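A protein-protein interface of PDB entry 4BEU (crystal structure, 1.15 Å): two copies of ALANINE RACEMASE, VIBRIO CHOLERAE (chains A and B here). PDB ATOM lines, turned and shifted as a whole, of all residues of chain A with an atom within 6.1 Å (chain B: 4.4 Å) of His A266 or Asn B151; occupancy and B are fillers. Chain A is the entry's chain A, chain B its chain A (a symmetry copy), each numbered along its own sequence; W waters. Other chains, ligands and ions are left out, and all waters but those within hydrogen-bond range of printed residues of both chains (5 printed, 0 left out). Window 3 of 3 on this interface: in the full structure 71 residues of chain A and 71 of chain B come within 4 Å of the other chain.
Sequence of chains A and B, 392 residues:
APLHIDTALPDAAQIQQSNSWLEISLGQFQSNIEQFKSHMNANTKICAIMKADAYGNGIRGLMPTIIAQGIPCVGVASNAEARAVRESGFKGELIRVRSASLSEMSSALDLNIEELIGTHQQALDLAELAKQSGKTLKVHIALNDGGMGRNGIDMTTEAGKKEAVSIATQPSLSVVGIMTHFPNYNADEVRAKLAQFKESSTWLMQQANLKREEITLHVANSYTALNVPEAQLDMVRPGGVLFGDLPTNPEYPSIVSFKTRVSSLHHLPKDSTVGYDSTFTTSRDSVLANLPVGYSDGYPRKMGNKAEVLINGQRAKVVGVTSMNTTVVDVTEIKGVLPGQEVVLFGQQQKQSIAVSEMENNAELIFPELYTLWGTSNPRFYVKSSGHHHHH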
ATOM      1  N   SER A 264     -17.069  18.369 -30.219  1.00  0.00           N
ATOM      2  CA  SER A 264     -16.352  18.165 -28.969  1.00  0.00           C
ATOM      3  C   SER A 264     -15.976  19.510 -28.372  1.00  0.00           C
ATOM      4  O   SER A 264     -15.893  20.510 -29.063  1.00  0.00           O
ATOM      5  CB  SER A 264     -15.129  17.254 -29.187  1.00  0.00           C
ATOM      6  OG  SER A 264     -14.319  17.685 -30.267  1.00  0.00           O
ATOM      7  N   LEU A 265     -15.761  19.501 -27.052  1.00  0.00           N
ATOM      8  CA  LEU A 265     -15.447  20.707 -26.285  1.00  0.00           C
ATOM      9  C   LEU A 265     -14.111  20.473 -25.588  1.00  0.00           C
ATOM     10  O   LEU A 265     -13.981  19.514 -24.832  1.00  0.00           O
ATOM     11  CB  LEU A 265     -16.536  21.012 -25.244  1.00  0.00           C
ATOM     12  CG  LEU A 265     -17.853  21.501 -25.834  1.00  0.00           C
ATOM     13  CD1 LEU A 265     -18.954  21.538 -24.770  1.00  0.00           C
ATOM     14  CD2 LEU A 265     -17.684  22.873 -26.468  1.00  0.00           C
ATOM     15  N   HIS A 266     -13.153  21.356 -25.832  1.00  0.00           N
ATOM     16  CA  HIS A 266     -11.786  21.166 -25.396  1.00  0.00           C
ATOM     17  C   HIS A 266     -11.347  22.309 -24.495  1.00  0.00           C
ATOM     18  O   HIS A 266     -11.490  23.476 -24.822  1.00  0.00           O
ATOM     19  CB  HIS A 266     -10.877  21.161 -26.622  1.00  0.00           C
ATOM     20  CG  HIS A 266     -11.221  20.101 -27.623  1.00  0.00           C
ATOM     21  ND1 HIS A 266     -10.436  18.993 -27.832  1.00  0.00           N
ATOM     22  CD2 HIS A 266     -12.273  19.977 -28.466  1.00  0.00           C
ATOM     23  CE1 HIS A 266     -10.995  18.226 -28.752  1.00  0.00           C
ATOM     24  NE2 HIS A 266     -12.112  18.800 -29.148  1.00  0.00           N
ATOM     25  N   HIS A 267     -10.746  21.964 -23.365  1.00  0.00           N
ATOM     26  CA  HIS A 267     -10.173  22.958 -22.442  1.00  0.00           C
ATOM     27  C   HIS A 267      -8.726  23.244 -22.813  1.00  0.00           C
ATOM     28  O   HIS A 267      -7.903  22.322 -22.867  1.00  0.00           O
ATOM     29  CB  HIS A 267     -10.263  22.457 -20.997  1.00  0.00           C
ATOM     30  CG  HIS A 267     -11.665  22.382 -20.475  1.00  0.00           C
ATOM     31  ND1 HIS A 267     -12.597  21.487 -20.956  1.00  0.00           N
ATOM     32  CD2 HIS A 267     -12.301  23.112 -19.527  1.00  0.00           C
ATOM     33  CE1 HIS A 267     -13.743  21.661 -20.321  1.00  0.00           C
ATOM     34  NE2 HIS A 267     -13.588  22.637 -19.444  1.00  0.00           N
ATOM     35  N   LEU A 268      -8.413  24.512 -23.053  1.00  0.00           N
ATOM     36  CA  LEU A 268      -7.072  24.948 -23.411  1.00  0.00           C
ATOM     37  C   LEU A 268      -6.657  26.084 -22.501  1.00  0.00           C
ATOM     38  O   LEU A 268      -7.380  27.090 -22.410  1.00  0.00           O
ATOM     39  CB  LEU A 268      -7.050  25.510 -24.821  1.00  0.00           C
ATOM     40  CG  LEU A 268      -6.710  24.632 -26.018  1.00  0.00           C
ATOM     41  CD1 LEU A 268      -6.371  25.552 -27.177  1.00  0.00           C
ATOM     42  CD2 LEU A 268      -5.547  23.689 -25.756  1.00  0.00           C
ATOM     43  N   SER A 286      -9.488  28.675 -21.638  1.00  0.00           N
ATOM     44  CA  SER A 286     -10.554  28.710 -22.631  1.00  0.00           C
ATOM     45  C   SER A 286     -11.268  27.371 -22.752  1.00  0.00           C
ATOM     46  O   SER A 286     -10.724  26.320 -22.410  1.00  0.00           O
ATOM     47  CB  SER A 286      -9.956  29.075 -23.990  1.00  0.00           C
ATOM     48  OG  SER A 286      -9.278  30.332 -23.941  1.00  0.00           O
ATOM     49  N   VAL A 287     -12.490  27.430 -23.270  1.00  0.00           N
ATOM     50  CA  VAL A 287     -13.183  26.241 -23.746  1.00  0.00           C
ATOM     51  C   VAL A 287     -13.450  26.477 -25.222  1.00  0.00           C
ATOM     52  O   VAL A 287     -14.079  27.471 -25.594  1.00  0.00           O
ATOM     53  CB  VAL A 287     -14.489  25.974 -22.988  1.00  0.00           C
ATOM     54  CG1 VAL A 287     -15.157  24.700 -23.508  1.00  0.00           C
ATOM     55  CG2 VAL A 287     -14.223  25.865 -21.485  1.00  0.00           C
ATOM     56  N   LEU A 288     -12.921  25.587 -26.060  1.00  0.00           N
ATOM     57  CA  LEU A 288     -13.078  25.680 -27.509  1.00  0.00           C
ATOM     58  C   LEU A 288     -14.015  24.603 -28.015  1.00  0.00           C
ATOM     59  O   LEU A 288     -13.905  23.441 -27.627  1.00  0.00           O
ATOM     60  CB  LEU A 288     -11.713  25.560 -28.183  1.00  0.00           C
ATOM     61  CG  LEU A 288     -10.705  26.611 -27.680  1.00  0.00           C
ATOM     62  CD1 LEU A 288      -9.396  26.481 -28.420  1.00  0.00           C
ATOM     63  CD2 LEU A 288     -11.218  28.037 -27.788  1.00  0.00           C
ATOM     64  N   ALA A 289     -14.941  24.994 -28.884  1.00  0.00           N
ATOM     65  CA  ALA A 289     -15.798  24.047 -29.594  1.00  0.00           C
ATOM     66  C   ALA A 289     -15.175  23.652 -30.935  1.00  0.00           C
ATOM     67  O   ALA A 289     -14.776  24.497 -31.729  1.00  0.00           O
ATOM     68  CB  ALA A 289     -17.166  24.651 -29.812  1.00  0.00           C
ATOM     69  N   ASN A 290     -15.052  22.348 -31.133  1.00  0.00           N
ATOM     70  CA  ASN A 290     -14.515  21.765 -32.350  1.00  0.00           C
ATOM     71  C   ASN A 290     -15.675  21.396 -33.244  1.00  0.00           C
ATOM     72  O   ASN A 290     -16.537  20.636 -32.836  1.00  0.00           O
ATOM     73  CB  ASN A 290     -13.681  20.556 -31.918  1.00  0.00           C
ATOM     74  CG  ASN A 290     -13.088  19.798 -33.072  1.00  0.00           C
ATOM     75  OD1 ASN A 290     -13.753  19.552 -34.075  1.00  0.00           O
ATOM     76  ND2 ASN A 290     -11.839  19.391 -32.929  1.00  0.00           N
ATOM     77  N   THR A 326     -12.066  21.083 -40.317  1.00  0.00           N
ATOM     78  CA  THR A 326     -12.388  21.417 -38.928  1.00  0.00           C
ATOM     79  C   THR A 326     -12.216  22.905 -38.665  1.00  0.00           C
ATOM     80  O   THR A 326     -11.321  23.527 -39.191  1.00  0.00           O
ATOM     81  CB  THR A 326     -11.453  20.624 -37.990  1.00  0.00           C
ATOM     82  OG1 THR A 326     -11.660  19.224 -38.202  1.00  0.00           O
ATOM     83  CG2 THR A 326     -11.617  20.967 -36.520  1.00  0.00           C
ATOM     84  N   VAL B  97      -9.393  11.321 -39.123  1.00  0.00           N
ATOM     85  CA  VAL B  97      -8.380  12.316 -38.800  1.00  0.00           C
ATOM     86  C   VAL B  97      -8.917  13.583 -38.155  1.00  0.00           C
ATOM     87  O   VAL B  97      -8.177  14.566 -38.013  1.00  0.00           O
ATOM     88  CB  VAL B  97      -7.503  12.666 -40.020  1.00  0.00           C
ATOM     89  CG1 VAL B  97      -6.777  11.423 -40.522  1.00  0.00           C
ATOM     90  CG2 VAL B  97      -8.336  13.272 -41.111  1.00  0.00           C
ATOM     91  N   ARG B  98     -10.177  13.584 -37.729  1.00  0.00           N
ATOM     92  CA  ARG B  98     -10.746  14.700 -37.014  1.00  0.00           C
ATOM     93  C   ARG B  98     -11.722  14.202 -35.972  1.00  0.00           C
ATOM     94  O   ARG B  98     -12.236  13.078 -36.055  1.00  0.00           O
ATOM     95  CB  ARG B  98     -11.458  15.660 -37.979  1.00  0.00           C
ATOM     96  CG  ARG B  98     -12.599  15.051 -38.775  1.00  0.00           C
ATOM     97  CD  ARG B  98     -13.580  16.112 -39.192  1.00  0.00           C
ATOM     98  NE  ARG B  98     -14.621  15.669 -40.127  1.00  0.00           N
ATOM     99  CZ  ARG B  98     -15.725  15.017 -39.781  1.00  0.00           C
ATOM    100  NH1 ARG B  98     -15.950  14.664 -38.526  1.00  0.00           N
ATOM    101  NH2 ARG B  98     -16.617  14.731 -40.704  1.00  0.00           N
ATOM    102  N   SER B  99     -12.007  15.072 -35.008  1.00  0.00           N
ATOM    103  CA  SER B  99     -13.155  14.913 -34.138  1.00  0.00           C
ATOM    104  C   SER B  99     -14.419  14.746 -34.982  1.00  0.00           C
ATOM    105  O   SER B  99     -14.603  15.445 -35.983  1.00  0.00           O
ATOM    106  CB  SER B  99     -13.281  16.136 -33.226  1.00  0.00           C
ATOM    107  OG  SER B  99     -14.398  15.964 -32.383  1.00  0.00           O
ATOM    108  N   LEU B 116     -10.681   9.344 -33.424  1.00  0.00           N
ATOM    109  CA  LEU B 116      -9.608  10.190 -32.920  1.00  0.00           C
ATOM    110  C   LEU B 116     -10.182  11.038 -31.821  1.00  0.00           C
ATOM    111  O   LEU B 116     -11.001  11.932 -32.089  1.00  0.00           O
ATOM    112  CB  LEU B 116      -9.122  11.120 -34.026  1.00  0.00           C
ATOM    113  CG  LEU B 116      -7.942  12.021 -33.639  1.00  0.00           C
ATOM    114  CD1 LEU B 116      -6.706  11.211 -33.331  1.00  0.00           C
ATOM    115  CD2 LEU B 116      -7.654  13.031 -34.730  1.00  0.00           C
ATOM    116  N   ILE B 117      -9.784  10.785 -30.582  1.00  0.00           N
ATOM    117  CA  ILE B 117     -10.436  11.458 -29.466  1.00  0.00           C
ATOM    118  C   ILE B 117      -9.483  12.262 -28.608  1.00  0.00           C
ATOM    119  O   ILE B 117      -8.300  11.915 -28.429  1.00  0.00           O
ATOM    120  CB  ILE B 117     -11.233  10.480 -28.638  1.00  0.00           C
ATOM    121  CG1 ILE B 117     -10.302   9.482 -27.986  1.00  0.00           C
ATOM    122  CG2 ILE B 117     -12.287   9.782 -29.514  1.00  0.00           C
ATOM    123  CD1 ILE B 117     -11.023   8.459 -27.129  1.00  0.00           C
ATOM    124  N   GLY B 118      -9.995  13.372 -28.110  1.00  0.00           N
ATOM    125  CA  GLY B 118      -9.211  14.292 -27.326  1.00  0.00           C
ATOM    126  C   GLY B 118      -9.943  14.849 -26.119  1.00  0.00           C
ATOM    127  O   GLY B 118      -9.456  15.800 -25.508  1.00  0.00           O
ATOM    128  N   THR B 119     -11.095  14.276 -25.774  1.00  0.00           N
ATOM    129  CA  THR B 119     -11.887  14.717 -24.628  1.00  0.00           C
ATOM    130  C   THR B 119     -12.521  13.537 -23.933  1.00  0.00           C
ATOM    131  O   THR B 119     -12.773  12.499 -24.510  1.00  0.00           O
ATOM    132  CB  THR B 119     -13.023  15.675 -25.025  1.00  0.00           C
ATOM    133  OG1 THR B 119     -14.035  14.970 -25.764  1.00  0.00           O
ATOM    134  CG2 THR B 119     -12.504  16.852 -25.832  1.00  0.00           C
ATOM    135  N   ALA B 142      -5.552  11.801 -29.393  1.00  0.00           N
ATOM    136  CA  ALA B 142      -4.876  12.985 -29.891  1.00  0.00           C
ATOM    137  C   ALA B 142      -4.363  13.798 -28.710  1.00  0.00           C
ATOM    138  O   ALA B 142      -5.143  14.191 -27.841  1.00  0.00           O
ATOM    139  CB  ALA B 142      -5.836  13.826 -30.720  1.00  0.00           C
ATOM    140  N   ARG B 150      -6.716  21.746 -31.392  1.00  0.00           N
ATOM    141  CA  ARG B 150      -7.768  21.358 -32.341  1.00  0.00           C
ATOM    142  C   ARG B 150      -8.478  20.075 -31.879  1.00  0.00           C
ATOM    143  O   ARG B 150      -9.476  20.162 -31.173  1.00  0.00           O
ATOM    144  CB  ARG B 150      -7.186  21.263 -33.755  1.00  0.00           C
ATOM    145  CG  ARG B 150      -8.208  21.040 -34.866  1.00  0.00           C
ATOM    146  CD  ARG B 150      -7.565  21.103 -36.257  1.00  0.00           C
ATOM    147  NE  ARG B 150      -6.660  19.974 -36.456  1.00  0.00           N
ATOM    148  CZ  ARG B 150      -6.186  19.607 -37.629  1.00  0.00           C
ATOM    149  NH1 ARG B 150      -6.461  20.298 -38.715  1.00  0.00           N
ATOM    150  NH2 ARG B 150      -5.422  18.528 -37.726  1.00  0.00           N
ATOM    151  N   ASN B 151      -7.980  18.898 -32.250  1.00  0.00           N
ATOM    152  CA  ASN B 151      -8.655  17.654 -31.888  1.00  0.00           C
ATOM    153  C   ASN B 151      -8.137  17.004 -30.596  1.00  0.00           C
ATOM    154  O   ASN B 151      -8.707  16.017 -30.127  1.00  0.00           O
ATOM    155  CB  ASN B 151      -8.486  16.627 -33.007  1.00  0.00           C
ATOM    156  CG  ASN B 151      -9.106  17.075 -34.297  1.00  0.00           C
ATOM    157  OD1 ASN B 151     -10.300  17.393 -34.358  1.00  0.00           O
ATOM    158  ND2 ASN B 151      -8.308  17.114 -35.346  1.00  0.00           N
ATOM    159  N   GLY B 152      -7.057  17.542 -30.016  1.00  0.00           N
ATOM    160  CA  GLY B 152      -6.364  16.873 -28.937  1.00  0.00           C
ATOM    161  C   GLY B 152      -6.671  17.320 -27.526  1.00  0.00           C
ATOM    162  O   GLY B 152      -7.396  18.284 -27.286  1.00  0.00           O
HETATM  163  O   HOH W   1     -13.627  18.164 -36.443  1.00  0.00           O
HETATM  164  O   HOH W   2      -9.073  18.345 -37.810  1.00  0.00           O
HETATM  165  O   HOH W   3     -16.263  16.751 -25.943  1.00  0.00           O
HETATM  166  O   HOH W   4      -7.376  20.335 -24.788  1.00  0.00           O
HETATM  167  O   HOH W   5      -9.523  18.517 -24.929  1.00  0.00           O
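Water W1 lies within hydrogen-bond range of OD1 of Asn A290 (2.7 Å), OG1 of Thr A326 (2.8 Å) and O of Ser B99 (2.9 Å). Water W2 lies within hydrogen-bond range of the side-chain hydroxyl (OG1) of Thr A326 (2.8 Å), the side-chain amide nitrogen (ND2) of Asn B151 (2.9 Å) and the guanidinium group (NE) of Arg B150 (3.2 Å). Water W5 lies within hydrogen-bond range of the backbone carbonyl oxygen (O) of Gly B118, a ring nitrogen (ND1) of His A266 and the backbone carbonyl oxygen (O) of Gly B152. Water W4 lies within hydrogen-bond range of the backbone carbonyl oxygen (O) of His A267 and the backbone carbonyl oxygen (O) of Gly B152. Water W3 bridges the side-chain hydroxyl of Thr B119 (2.9 Å) and the backbone NH of Leu A265 (3.0 Å).
The guanidinium group of Arg B150 lies close to the side-chain amide nitrogen of Asn B151 (3.5 Å). The backbone NH of Leu A288 sits at hydrogen-bond distance from the backbone carbonyl oxygen of His A266. The side-chain hydroxyl (OG) of Ser A264 is in hydrogen-bond range of a ring nitrogen (NE2) of His A266. The backbone carbonyl oxygen (O) of Ser A264 is in hydrogen-bond range of the backbone NH (N) of Asn A290, 2.9 Å away. The backbone NH (N) of Ser B99 sits at hydrogen-bond distance from the side-chain amide oxygen (OD1) of Asn B151 (3.0 Å).
No position is printed for both chains. Of the 11 pairs that touch across the chains among the printed residues, none has its exchanged pair printed and touching as well.
The side-chain hydroxyl of Ser A264 is in hydrogen-bond range of the side-chain hydroxyl of Ser B99 (2.7 Å). ND1 of His A266 is in hydrogen-bond range of O of Gly B152, 3.2 Å away. The side-chain amide nitrogen (ND2) of Asn A290 lies within hydrogen-bond range of the side-chain amide oxygen (OD1) of Asn B151 (2.9 Å). The backbone carbonyl oxygen of Arg B150 is in hydrogen-bond range of the side-chain amide nitrogen of Asn A290, at 3.0 Å.
His A266 touches just these residues of chain B: Thr B119, Arg B150, Asn B151 and Gly B152. Of the printed residues of chain B, Asn A290 touches Ser B99, Arg B150 and Asn B151. Of the printed residues of chain B, Thr A326 touches Arg B98 and Arg B150. Printed residues of chain A within 4 Å of Ser B99: Ser A264 (2.7 Å) and Asn A290 (3.6 Å). Leu B116 touches none of the printed residues of chain A. Asn B151 touches just these residues of chain A: His A266 (3.5 Å) and Asn A290 (2.9 Å). The nearest residue of chain B that does not touch His A266 is Gly B118 (4.1 Å). The nearest residue of chain A that does not touch Asn B151 is Thr A326 (4.4 Å). The nearest printed residue of chain A that does not touch Ser B99 is His A266 (4.9 Å).
Printed residues of chain A that touch a printed residue of chain B: Ser A264, Leu A265, His A266, Asn A290 and Thr A326. Hydrophobic or aromatic side chains of chain A within 4 Å of the printed part of chain B: His A266. Among the printed residues, 11 pairs touch across the chains.
Among the printed residues, pairs that only touch across the chains: Leu A265 with Thr B119 (3.2 Å), His A266 with Arg B150 (3.5 Å), His A266 with Asn B151 (3.5 Å), Asn A290 with Ser B99 (3.6 Å), His A266 with Thr B119 (3.6 Å), Thr A326 with Arg B98 (3.6 Å) and Thr A326 with Arg B150 (3.8 Å).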
